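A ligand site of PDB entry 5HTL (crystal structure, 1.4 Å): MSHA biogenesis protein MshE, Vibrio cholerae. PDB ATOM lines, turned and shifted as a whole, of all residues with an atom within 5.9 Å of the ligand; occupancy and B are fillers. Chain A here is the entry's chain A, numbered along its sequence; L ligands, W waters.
NE of Arg 9 sits close to N3 of the ligand, 3.4 Å away. Leu 25 touches the ligand (CD2 to O7, 3.5 Å). CD1 of Leu 29 touches C9 of the ligand, 3.5 Å away. Leu 54 touches the ligand. Leu 58 touches the ligand. Ala 110 touches the ligand. Hydrophobic or aromatic side chains within 4 Å of the ligand: Leu 10, Leu 25, Leu 29, Leu 39, Leu 54, Leu 58 and Ala 110. Within 4 Å of the ligand: Arg 7, Arg 9, Leu 10, Gly 11, Asp 12, Leu 25, Leu 29, Gln 32, Arg 38, Leu 39, Gly 40, Asp 41, Leu 54, Leu 58, Gln 61, Asp 108 and Ala 110. The nearest printed residue that does not touch the ligand is Lys 8 (4.3 Å).
Water W2 lies within hydrogen-bond range of an oxygen (O2) of the ligand (2.7 Å), the backbone carbonyl oxygen of Arg 7 (3.0 Å) and the backbone NH of Arg 9 (3.4 Å). Water W5 lies within hydrogen-bond range of a nitrogen (N9) of the ligand and the backbone carbonyl oxygen of Ser 107. Water W6 bridges OD2 of Asp 41 (2.6 Å) and N8 of the ligand (2.9 Å). Water W7 lies within hydrogen-bond range of the side-chain carboxylate (OD2) of Asp 108 (2.8 Å), a nitrogen (N10) of the ligand (3.2 Å) and the guanidinium group (NE) of Arg 38 (3.3 Å).
NE2 of Gln 61 lies close to N of Leu 10, at 3.3 Å. O of Lys 8 lies within hydrogen-bond range of NE2 of Gln 61 (2.8 Å). The side-chain amide nitrogen (NE2) of Gln 32 lies close to the backbone NH (N) of Leu 39 (3.0 Å). The side-chain amide nitrogen (NE2) of Gln 32 sits at hydrogen-bond distance from the backbone carbonyl oxygen (O) of Arg 37, 2.9 Å away. OD1 of Asp 108 sits close to N of Ala 110, 3.1 Å away. The backbone carbonyl oxygen (O) of Arg 38 sits at hydrogen-bond distance from the side-chain hydroxyl (OG1) of Thr 42 (2.9 Å). OD2 of Asp 12 lies within salt-bridge range of NE of Arg 9 (2.7 Å).
OE1 of Gln 61 lies within hydrogen-bond range of O13 of the ligand (2.7 Å). O1 of the ligand lies within hydrogen-bond range of N of Leu 10, at 2.7 Å. An oxygen (O14) of the ligand lies within hydrogen-bond range of the backbone NH (N) of Asp 41 (2.7 Å). The backbone NH of Leu 39 lies within hydrogen-bond range of an oxygen (O9) of the ligand (2.8 Å). An oxygen (O9) of the ligand is in hydrogen-bond range of the side-chain amide nitrogen (NE2) of Gln 32 (2.9 Å). The side-chain carboxylate (OD1) of Asp 108 is in hydrogen-bond range of a nitrogen (N9) of the ligand, 2.9 Å away. An oxygen (O13) of the ligand sits at hydrogen-bond distance from the guanidinium group (NH1) of Arg 7. The guanidinium group of Arg 38 is in salt-bridge range of an oxygen (O8) of the ligand (3.0 Å). N of Asp 12 is in hydrogen-bond range of O7 of the ligand (3.0 Å). The backbone NH (N) of Gly 40 lies within hydrogen-bond range of a nitrogen (N7) of the ligand. N2 of the ligand sits at hydrogen-bond distance from N of Gly 11.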
ATOM      1  N   ARG A   7      -1.567  -7.302 -15.144  1.00  0.00           N
ATOM      2  CA  ARG A   7      -2.740  -7.235 -15.992  1.00  0.00           C
ATOM      3  C   ARG A   7      -3.157  -5.768 -16.093  1.00  0.00           C
ATOM      4  O   ARG A   7      -2.721  -4.934 -15.294  1.00  0.00           O
ATOM      5  CB  ARG A   7      -3.859  -8.014 -15.312  1.00  0.00           C
ATOM      6  CG  ARG A   7      -4.226  -7.413 -13.967  1.00  0.00           C
ATOM      7  CD  ARG A   7      -5.003  -8.363 -13.102  1.00  0.00           C
ATOM      8  NE  ARG A   7      -4.132  -9.414 -12.589  1.00  0.00           N
ATOM      9  CZ  ARG A   7      -4.476 -10.271 -11.646  1.00  0.00           C
ATOM     10  NH1 ARG A   7      -5.694 -10.206 -11.101  1.00  0.00           N
ATOM     11  NH2 ARG A   7      -3.612 -11.191 -11.238  1.00  0.00           N
ATOM     12  N   LYS A   8      -3.987  -5.466 -17.081  1.00  0.00           N
ATOM     13  CA  LYS A   8      -4.620  -4.161 -17.126  1.00  0.00           C
ATOM     14  C   LYS A   8      -5.721  -4.204 -16.072  1.00  0.00           C
ATOM     15  O   LYS A   8      -6.455  -5.181 -16.004  1.00  0.00           O
ATOM     16  CB  LYS A   8      -5.218  -3.914 -18.506  1.00  0.00           C
ATOM     17  CG  LYS A   8      -5.897  -2.578 -18.638  1.00  0.00           C
ATOM     18  CD  LYS A   8      -6.584  -2.453 -19.978  1.00  0.00           C
ATOM     19  CE  LYS A   8      -7.198  -1.082 -20.108  1.00  0.00           C
ATOM     20  NZ  LYS A   8      -6.143  -0.031 -20.048  1.00  0.00           N
ATOM     21  N   ARG A   9      -5.845  -3.179 -15.244  1.00  0.00           N
ATOM     22  CA  ARG A   9      -6.852  -3.268 -14.193  1.00  0.00           C
ATOM     23  C   ARG A   9      -8.263  -3.252 -14.771  1.00  0.00           C
ATOM     24  O   ARG A   9      -8.523  -2.677 -15.847  1.00  0.00           O
ATOM     25  CB  ARG A   9      -6.653  -2.244 -13.078  1.00  0.00           C
ATOM     26  CG  ARG A   9      -6.740  -0.817 -13.513  1.00  0.00           C
ATOM     27  CD  ARG A   9      -6.315   0.102 -12.379  1.00  0.00           C
ATOM     28  NE  ARG A   9      -6.524   1.475 -12.753  1.00  0.00           N
ATOM     29  CZ  ARG A   9      -6.257   2.507 -11.965  1.00  0.00           C
ATOM     30  NH1 ARG A   9      -5.769   2.312 -10.748  1.00  0.00           N
ATOM     31  NH2 ARG A   9      -6.476   3.738 -12.402  1.00  0.00           N
ATOM     32  N   LEU A  10      -9.190  -3.906 -14.067  1.00  0.00           N
ATOM     33  CA  LEU A  10     -10.479  -4.243 -14.625  1.00  0.00           C
ATOM     34  C   LEU A  10     -11.341  -3.036 -14.963  1.00  0.00           C
ATOM     35  O   LEU A  10     -11.974  -3.015 -16.012  1.00  0.00           O
ATOM     36  CB  LEU A  10     -11.232  -5.206 -13.701  1.00  0.00           C
ATOM     37  CG  LEU A  10     -12.553  -5.728 -14.255  1.00  0.00           C
ATOM     38  CD1 LEU A  10     -12.319  -6.559 -15.498  1.00  0.00           C
ATOM     39  CD2 LEU A  10     -13.277  -6.530 -13.185  1.00  0.00           C
ATOM     40  N   GLY A  11     -11.359  -2.030 -14.089  1.00  0.00           N
ATOM     41  CA  GLY A  11     -12.143  -0.827 -14.348  1.00  0.00           C
ATOM     42  C   GLY A  11     -11.766  -0.164 -15.667  1.00  0.00           C
ATOM     43  O   GLY A  11     -12.626   0.069 -16.522  1.00  0.00           O
ATOM     44  N   ASP A  12     -10.477   0.127 -15.842  1.00  0.00           N
ATOM     45  CA  ASP A  12      -9.991   0.751 -17.064  1.00  0.00           C
ATOM     46  C   ASP A  12     -10.303  -0.096 -18.285  1.00  0.00           C
ATOM     47  O   ASP A  12     -10.657   0.444 -19.331  1.00  0.00           O
ATOM     48  CB  ASP A  12      -8.488   1.013 -16.983  1.00  0.00           C
ATOM     49  CG  ASP A  12      -8.140   2.039 -15.923  1.00  0.00           C
ATOM     50  OD1 ASP A  12      -8.951   2.963 -15.686  1.00  0.00           O
ATOM     51  OD2 ASP A  12      -7.052   1.925 -15.325  1.00  0.00           O
ATOM     52  N   LEU A  13     -10.194  -1.413 -18.158  1.00  0.00           N
ATOM     53  CA  LEU A  13     -10.514  -2.304 -19.273  1.00  0.00           C
ATOM     54  C   LEU A  13     -11.982  -2.155 -19.670  1.00  0.00           C
ATOM     55  O   LEU A  13     -12.320  -2.021 -20.850  1.00  0.00           O
ATOM     56  CB  LEU A  13     -10.206  -3.754 -18.860  1.00  0.00           C
ATOM     57  CG  LEU A  13     -10.396  -4.880 -19.886  1.00  0.00           C
ATOM     58  CD1 LEU A  13      -9.546  -6.060 -19.491  1.00  0.00           C
ATOM     59  CD2 LEU A  13     -11.833  -5.329 -19.945  1.00  0.00           C
ATOM     60  N   LEU A  25     -17.740   3.756 -12.944  1.00  0.00           N
ATOM     61  CA  LEU A  25     -16.540   3.186 -12.357  1.00  0.00           C
ATOM     62  C   LEU A  25     -16.205   3.896 -11.045  1.00  0.00           C
ATOM     63  O   LEU A  25     -15.953   3.237 -10.038  1.00  0.00           O
ATOM     64  CB  LEU A  25     -15.364   3.282 -13.314  1.00  0.00           C
ATOM     65  CG  LEU A  25     -14.017   2.793 -12.772  1.00  0.00           C
ATOM     66  CD1 LEU A  25     -14.072   1.372 -12.171  1.00  0.00           C
ATOM     67  CD2 LEU A  25     -12.952   2.855 -13.858  1.00  0.00           C
ATOM     68  N   LEU A  29     -16.072   2.184  -7.344  1.00  0.00           N
ATOM     69  CA  LEU A  29     -14.852   2.200  -6.538  1.00  0.00           C
ATOM     70  C   LEU A  29     -15.138   2.794  -5.168  1.00  0.00           C
ATOM     71  O   LEU A  29     -14.654   2.273  -4.157  1.00  0.00           O
ATOM     72  CB  LEU A  29     -13.735   2.957  -7.248  1.00  0.00           C
ATOM     73  CG  LEU A  29     -13.150   2.257  -8.468  1.00  0.00           C
ATOM     74  CD1 LEU A  29     -12.271   3.243  -9.231  1.00  0.00           C
ATOM     75  CD2 LEU A  29     -12.348   1.019  -8.052  1.00  0.00           C
ATOM     76  N   GLN A  32     -17.355   0.160  -3.203  1.00  0.00           N
ATOM     77  CA  GLN A  32     -16.715  -1.109  -2.885  1.00  0.00           C
ATOM     78  C   GLN A  32     -15.976  -1.078  -1.540  1.00  0.00           C
ATOM     79  O   GLN A  32     -15.872  -2.099  -0.848  1.00  0.00           O
ATOM     80  CB  GLN A  32     -15.757  -1.478  -4.035  1.00  0.00           C
ATOM     81  CG  GLN A  32     -14.497  -2.187  -3.607  1.00  0.00           C
ATOM     82  CD  GLN A  32     -13.613  -2.554  -4.785  1.00  0.00           C
ATOM     83  OE1 GLN A  32     -13.033  -1.693  -5.440  1.00  0.00           O
ATOM     84  NE2 GLN A  32     -13.484  -3.839  -5.028  1.00  0.00           N
ATOM     85  N   ARG A  37     -16.254  -6.799  -1.054  1.00  0.00           N
ATOM     86  CA  ARG A  37     -16.641  -7.189  -2.410  1.00  0.00           C
ATOM     87  C   ARG A  37     -15.652  -6.672  -3.453  1.00  0.00           C
ATOM     88  O   ARG A  37     -15.103  -5.587  -3.322  1.00  0.00           O
ATOM     89  CB  ARG A  37     -18.068  -6.732  -2.711  1.00  0.00           C
ATOM     90  CG  ARG A  37     -19.098  -7.332  -1.756  1.00  0.00           C
ATOM     91  CD  ARG A  37     -20.313  -7.912  -2.474  1.00  0.00           C
ATOM     92  NE  ARG A  37     -20.921  -8.991  -1.699  1.00  0.00           N
ATOM     93  CZ  ARG A  37     -21.807  -8.824  -0.730  1.00  0.00           C
ATOM     94  NH1 ARG A  37     -22.300  -9.875  -0.089  1.00  0.00           N
ATOM     95  NH2 ARG A  37     -22.211  -7.611  -0.384  1.00  0.00           N
ATOM     96  N   ARG A  38     -15.401  -7.489  -4.463  1.00  0.00           N
ATOM     97  CA  ARG A  38     -14.528  -7.057  -5.545  1.00  0.00           C
ATOM     98  C   ARG A  38     -15.256  -6.103  -6.503  1.00  0.00           C
ATOM     99  O   ARG A  38     -16.477  -5.940  -6.422  1.00  0.00           O
ATOM    100  CB  ARG A  38     -13.911  -8.262  -6.251  1.00  0.00           C
ATOM    101  CG  ARG A  38     -13.157  -9.170  -5.278  1.00  0.00           C
ATOM    102  CD  ARG A  38     -11.906  -9.762  -5.907  1.00  0.00           C
ATOM    103  NE  ARG A  38     -11.265 -10.730  -5.018  1.00  0.00           N
ATOM    104  CZ  ARG A  38     -10.248 -10.454  -4.194  1.00  0.00           C
ATOM    105  NH1 ARG A  38      -9.710  -9.239  -4.144  1.00  0.00           N
ATOM    106  NH2 ARG A  38      -9.760 -11.422  -3.441  1.00  0.00           N
ATOM    107  N   LEU A  39     -14.492  -5.476  -7.392  1.00  0.00           N
ATOM    108  CA  LEU A  39     -15.033  -4.430  -8.237  1.00  0.00           C
ATOM    109  C   LEU A  39     -16.109  -4.908  -9.206  1.00  0.00           C
ATOM    110  O   LEU A  39     -17.145  -4.256  -9.360  1.00  0.00           O
ATOM    111  CB  LEU A  39     -13.915  -3.739  -9.025  1.00  0.00           C
ATOM    112  CG  LEU A  39     -14.352  -2.669 -10.022  1.00  0.00           C
ATOM    113  CD1 LEU A  39     -15.095  -1.520  -9.336  1.00  0.00           C
ATOM    114  CD2 LEU A  39     -13.139  -2.176 -10.789  1.00  0.00           C
ATOM    115  N   GLY A  40     -15.872  -6.045  -9.852  1.00  0.00           N
ATOM    116  CA  GLY A  40     -16.820  -6.581 -10.813  1.00  0.00           C
ATOM    117  C   GLY A  40     -18.172  -6.838 -10.162  1.00  0.00           C
ATOM    118  O   GLY A  40     -19.221  -6.426 -10.686  1.00  0.00           O
ATOM    119  N   ASP A  41     -18.157  -7.513  -9.024  1.00  0.00           N
ATOM    120  CA  ASP A  41     -19.390  -7.808  -8.287  1.00  0.00           C
ATOM    121  C   ASP A  41     -20.080  -6.518  -7.814  1.00  0.00           C
ATOM    122  O   ASP A  41     -21.306  -6.441  -7.750  1.00  0.00           O
ATOM    123  CB  ASP A  41     -19.100  -8.768  -7.133  1.00  0.00           C
ATOM    124  CG  ASP A  41     -18.853 -10.200  -7.608  1.00  0.00           C
ATOM    125  OD1 ASP A  41     -19.380 -10.607  -8.672  1.00  0.00           O
ATOM    126  OD2 ASP A  41     -18.137 -10.948  -6.890  1.00  0.00           O
ATOM    127  N   THR A  42     -19.295  -5.482  -7.502  1.00  0.00           N
ATOM    128  CA  THR A  42     -19.881  -4.188  -7.144  1.00  0.00           C
ATOM    129  C   THR A  42     -20.591  -3.549  -8.345  1.00  0.00           C
ATOM    130  O   THR A  42     -21.716  -3.047  -8.222  1.00  0.00           O
ATOM    131  CB  THR A  42     -18.828  -3.239  -6.559  1.00  0.00           C
ATOM    132  OG1 THR A  42     -18.228  -3.858  -5.418  1.00  0.00           O
ATOM    133  CG2 THR A  42     -19.476  -1.948  -6.114  1.00  0.00           C
ATOM    134  N   ILE A  44     -21.813  -5.173 -10.862  1.00  0.00           N
ATOM    135  CA  ILE A  44     -23.015  -5.985 -11.102  1.00  0.00           C
ATOM    136  C   ILE A  44     -24.142  -5.614 -10.142  1.00  0.00           C
ATOM    137  O   ILE A  44     -25.301  -5.484 -10.537  1.00  0.00           O
ATOM    138  CB  ILE A  44     -22.706  -7.488 -10.974  1.00  0.00           C
ATOM    139  CG1 ILE A  44     -21.821  -7.937 -12.126  1.00  0.00           C
ATOM    140  CG2 ILE A  44     -24.003  -8.304 -10.967  1.00  0.00           C
ATOM    141  CD1 ILE A  44     -21.308  -9.355 -11.965  1.00  0.00           C
ATOM    142  N   LEU A  54     -18.911  -9.815 -16.983  1.00  0.00           N
ATOM    143  CA  LEU A  54     -17.782  -9.977 -16.065  1.00  0.00           C
ATOM    144  C   LEU A  54     -16.923 -11.185 -16.412  1.00  0.00           C
ATOM    145  O   LEU A  54     -15.692 -11.090 -16.456  1.00  0.00           O
ATOM    146  CB  LEU A  54     -18.266 -10.043 -14.612  1.00  0.00           C
ATOM    147  CG  LEU A  54     -17.166 -10.274 -13.560  1.00  0.00           C
ATOM    148  CD1 LEU A  54     -16.107  -9.159 -13.655  1.00  0.00           C
ATOM    149  CD2 LEU A  54     -17.756 -10.373 -12.156  1.00  0.00           C
ATOM    150  N   LEU A  58     -13.069 -10.667 -17.474  1.00  0.00           N
ATOM    151  CA  LEU A  58     -12.043 -11.293 -16.645  1.00  0.00           C
ATOM    152  C   LEU A  58     -11.177 -12.198 -17.526  1.00  0.00           C
ATOM    153  O   LEU A  58      -9.957 -12.190 -17.421  1.00  0.00           O
ATOM    154  CB  LEU A  58     -12.684 -12.115 -15.521  1.00  0.00           C
ATOM    155  CG  LEU A  58     -13.166 -11.323 -14.310  1.00  0.00           C
ATOM    156  CD1 LEU A  58     -13.901 -12.237 -13.330  1.00  0.00           C
ATOM    157  CD2 LEU A  58     -12.014 -10.620 -13.625  1.00  0.00           C
ATOM    158  N   GLN A  61      -8.919  -9.928 -19.497  1.00  0.00           N
ATOM    159  CA  GLN A  61      -7.911  -9.390 -18.585  1.00  0.00           C
ATOM    160  C   GLN A  61      -6.791 -10.378 -18.264  1.00  0.00           C
ATOM    161  O   GLN A  61      -5.607 -10.013 -18.237  1.00  0.00           O
ATOM    162  CB  GLN A  61      -8.576  -8.948 -17.276  1.00  0.00           C
ATOM    163  CG  GLN A  61      -7.584  -8.319 -16.310  1.00  0.00           C
ATOM    164  CD  GLN A  61      -8.145  -8.106 -14.925  1.00  0.00           C
ATOM    165  OE1 GLN A  61      -8.767  -9.004 -14.346  1.00  0.00           O
ATOM    166  NE2 GLN A  61      -7.927  -6.920 -14.375  1.00  0.00           N
ATOM    167  N   LEU A  62      -7.175 -11.618 -17.979  1.00  0.00           N
ATOM    168  CA  LEU A  62      -6.234 -12.649 -17.564  1.00  0.00           C
ATOM    169  C   LEU A  62      -5.635 -13.450 -18.717  1.00  0.00           C
ATOM    170  O   LEU A  62      -4.840 -14.374 -18.495  1.00  0.00           O
ATOM    171  CB  LEU A  62      -6.920 -13.586 -16.578  1.00  0.00           C
ATOM    172  CG  LEU A  62      -7.495 -12.882 -15.340  1.00  0.00           C
ATOM    173  CD1 LEU A  62      -8.238 -13.895 -14.465  1.00  0.00           C
ATOM    174  CD2 LEU A  62      -6.366 -12.159 -14.580  1.00  0.00           C
ATOM    175  N   SER A 107     -13.864 -21.089 -11.555  1.00  0.00           N
ATOM    176  CA  SER A 107     -14.856 -20.032 -11.588  1.00  0.00           C
ATOM    177  C   SER A 107     -14.174 -18.698 -11.348  1.00  0.00           C
ATOM    178  O   SER A 107     -14.614 -17.666 -11.847  1.00  0.00           O
ATOM    179  CB  SER A 107     -15.907 -20.267 -10.506  1.00  0.00           C
ATOM    180  OG  SER A 107     -15.412 -19.873  -9.252  1.00  0.00           O
ATOM    181  N   ASP A 108     -13.092 -18.709 -10.580  1.00  0.00           N
ATOM    182  CA  ASP A 108     -12.345 -17.475 -10.314  1.00  0.00           C
ATOM    183  C   ASP A 108     -10.837 -17.673 -10.425  1.00  0.00           C
ATOM    184  O   ASP A 108     -10.151 -17.876  -9.430  1.00  0.00           O
ATOM    185  CB  ASP A 108     -12.719 -16.915  -8.939  1.00  0.00           C
ATOM    186  CG  ASP A 108     -12.105 -15.558  -8.684  1.00  0.00           C
ATOM    187  OD1 ASP A 108     -11.482 -15.004  -9.597  1.00  0.00           O
ATOM    188  OD2 ASP A 108     -12.270 -15.053  -7.551  1.00  0.00           O
ATOM    189  N   PRO A 109     -10.299 -17.609 -11.650  1.00  0.00           N
ATOM    190  CA  PRO A 109      -8.851 -17.776 -11.813  1.00  0.00           C
ATOM    191  C   PRO A 109      -8.057 -16.582 -11.259  1.00  0.00           C
ATOM    192  O   PRO A 109      -6.840 -16.691 -11.105  1.00  0.00           O
ATOM    193  CB  PRO A 109      -8.674 -17.902 -13.329  1.00  0.00           C
ATOM    194  CG  PRO A 109      -9.939 -17.383 -13.920  1.00  0.00           C
ATOM    195  CD  PRO A 109     -11.016 -17.643 -12.927  1.00  0.00           C
ATOM    196  N   ALA A 110      -8.736 -15.495 -10.917  1.00  0.00           N
ATOM    197  CA  ALA A 110      -8.114 -14.338 -10.262  1.00  0.00           C
ATOM    198  C   ALA A 110      -7.956 -14.549  -8.744  1.00  0.00           C
ATOM    199  O   ALA A 110      -7.366 -13.711  -8.062  1.00  0.00           O
ATOM    200  CB  ALA A 110      -8.901 -13.076 -10.541  1.00  0.00           C
HETATM  201  P1  LIG L   1      -7.229  -5.587 -10.885  1.00  0.00           P
HETATM  202  O1  LIG L   1      -8.188  -5.399 -12.029  1.00  0.00           O
HETATM  203  O2  LIG L   1      -5.781  -5.431 -11.311  1.00  0.00           O
HETATM  204  O3  LIG L   1      -7.601  -4.531  -9.766  1.00  0.00           O
HETATM  205  C1  LIG L   1      -7.037  -4.463  -8.481  1.00  0.00           C
HETATM  206  C2  LIG L   1      -7.731  -3.571  -7.561  1.00  0.00           C
HETATM  207  O4  LIG L   1      -7.692  -2.259  -8.020  1.00  0.00           O
HETATM  208  C3  LIG L   1      -9.197  -3.917  -7.442  1.00  0.00           C
HETATM  209  O5  LIG L   1      -9.408  -4.774  -6.342  1.00  0.00           O
HETATM  210  C4  LIG L   1      -9.837  -2.687  -7.353  1.00  0.00           C
HETATM  211  O6  LIG L   1     -10.040  -2.319  -5.975  1.00  0.00           O
HETATM  212  C5  LIG L   1      -8.969  -1.688  -8.031  1.00  0.00           C
HETATM  213  N1  LIG L   1      -9.345  -1.511  -9.404  1.00  0.00           N
HETATM  214  C6  LIG L   1      -9.711  -2.278 -10.433  1.00  0.00           C
HETATM  215  N2  LIG L   1      -9.883  -1.445 -11.467  1.00  0.00           N
HETATM  216  C7  LIG L   1      -9.633  -0.162 -11.065  1.00  0.00           C
HETATM  217  C8  LIG L   1      -9.669   1.055 -11.756  1.00  0.00           C
HETATM  218  O7  LIG L   1     -10.018   1.097 -13.063  1.00  0.00           O
HETATM  219  N3  LIG L   1      -9.366   2.184 -11.103  1.00  0.00           N
HETATM  220  C9  LIG L   1      -9.020   2.133  -9.818  1.00  0.00           C
HETATM  221  N4  LIG L   1      -8.705   3.372  -9.179  1.00  0.00           N
HETATM  222  N5  LIG L   1      -8.965   0.983  -9.108  1.00  0.00           N
HETATM  223  C10 LIG L   1      -9.267  -0.188  -9.704  1.00  0.00           C
HETATM  224  P2  LIG L   1     -10.485  -5.940  -6.407  1.00  0.00           P
HETATM  225  O8  LIG L   1     -10.649  -6.572  -5.030  1.00  0.00           O
HETATM  226  O9  LIG L   1     -11.789  -5.325  -6.802  1.00  0.00           O
HETATM  227  O10 LIG L   1     -10.142  -6.984  -7.523  1.00  0.00           O
HETATM  228  C11 LIG L   1      -8.969  -7.765  -7.480  1.00  0.00           C
HETATM  229  C12 LIG L   1      -8.598  -8.417  -8.708  1.00  0.00           C
HETATM  230  O11 LIG L   1      -9.576  -9.464  -9.032  1.00  0.00           O
HETATM  231  C13 LIG L   1      -8.625  -7.516  -9.877  1.00  0.00           C
HETATM  232  O12 LIG L   1      -7.357  -7.032 -10.253  1.00  0.00           O
HETATM  233  C14 LIG L   1      -9.235  -8.296 -10.982  1.00  0.00           C
HETATM  234  O13 LIG L   1      -8.324  -8.999 -11.720  1.00  0.00           O
HETATM  235  C15 LIG L   1     -10.131  -9.279 -10.309  1.00  0.00           C
HETATM  236  N6  LIG L   1     -11.528  -8.906 -10.102  1.00  0.00           N
HETATM  237  C16 LIG L   1     -12.068  -7.685  -9.935  1.00  0.00           C
HETATM  238  N7  LIG L   1     -13.385  -7.804  -9.722  1.00  0.00           N
HETATM  239  C17 LIG L   1     -13.701  -9.120  -9.738  1.00  0.00           C
HETATM  240  C18 LIG L   1     -14.878  -9.867  -9.574  1.00  0.00           C
HETATM  241  O14 LIG L   1     -16.092  -9.265  -9.328  1.00  0.00           O
HETATM  242  N8  LIG L   1     -14.812 -11.193  -9.657  1.00  0.00           N
HETATM  243  C19 LIG L   1     -13.666 -11.824  -9.889  1.00  0.00           C
HETATM  244  N9  LIG L   1     -13.717 -13.225  -9.966  1.00  0.00           N
HETATM  245  N10 LIG L   1     -12.520 -11.158 -10.046  1.00  0.00           N
HETATM  246  C20 LIG L   1     -12.520  -9.809  -9.969  1.00  0.00           C
HETATM  247  O   HOH W   1      -3.650  -6.896  -9.971  1.00  0.00           O
HETATM  248  O   HOH W   2      -3.887  -4.046 -12.624  1.00  0.00           O
HETATM  249  O   HOH W   3      -4.866  -1.353  -8.564  1.00  0.00           O
HETATM  250  O   HOH W   4      -9.825   4.926 -12.174  1.00  0.00           O
HETATM  251  O   HOH W   5     -15.748 -14.912 -10.788  1.00  0.00           O
HETATM  252  O   HOH W   6     -16.623 -12.764  -8.021  1.00  0.00           O
HETATM  253  O   HOH W   7     -10.864 -12.612  -7.744  1.00  0.00           O
HETATM  254  O   HOH W   8      -8.682   3.814  -6.315  1.00  0.00           O
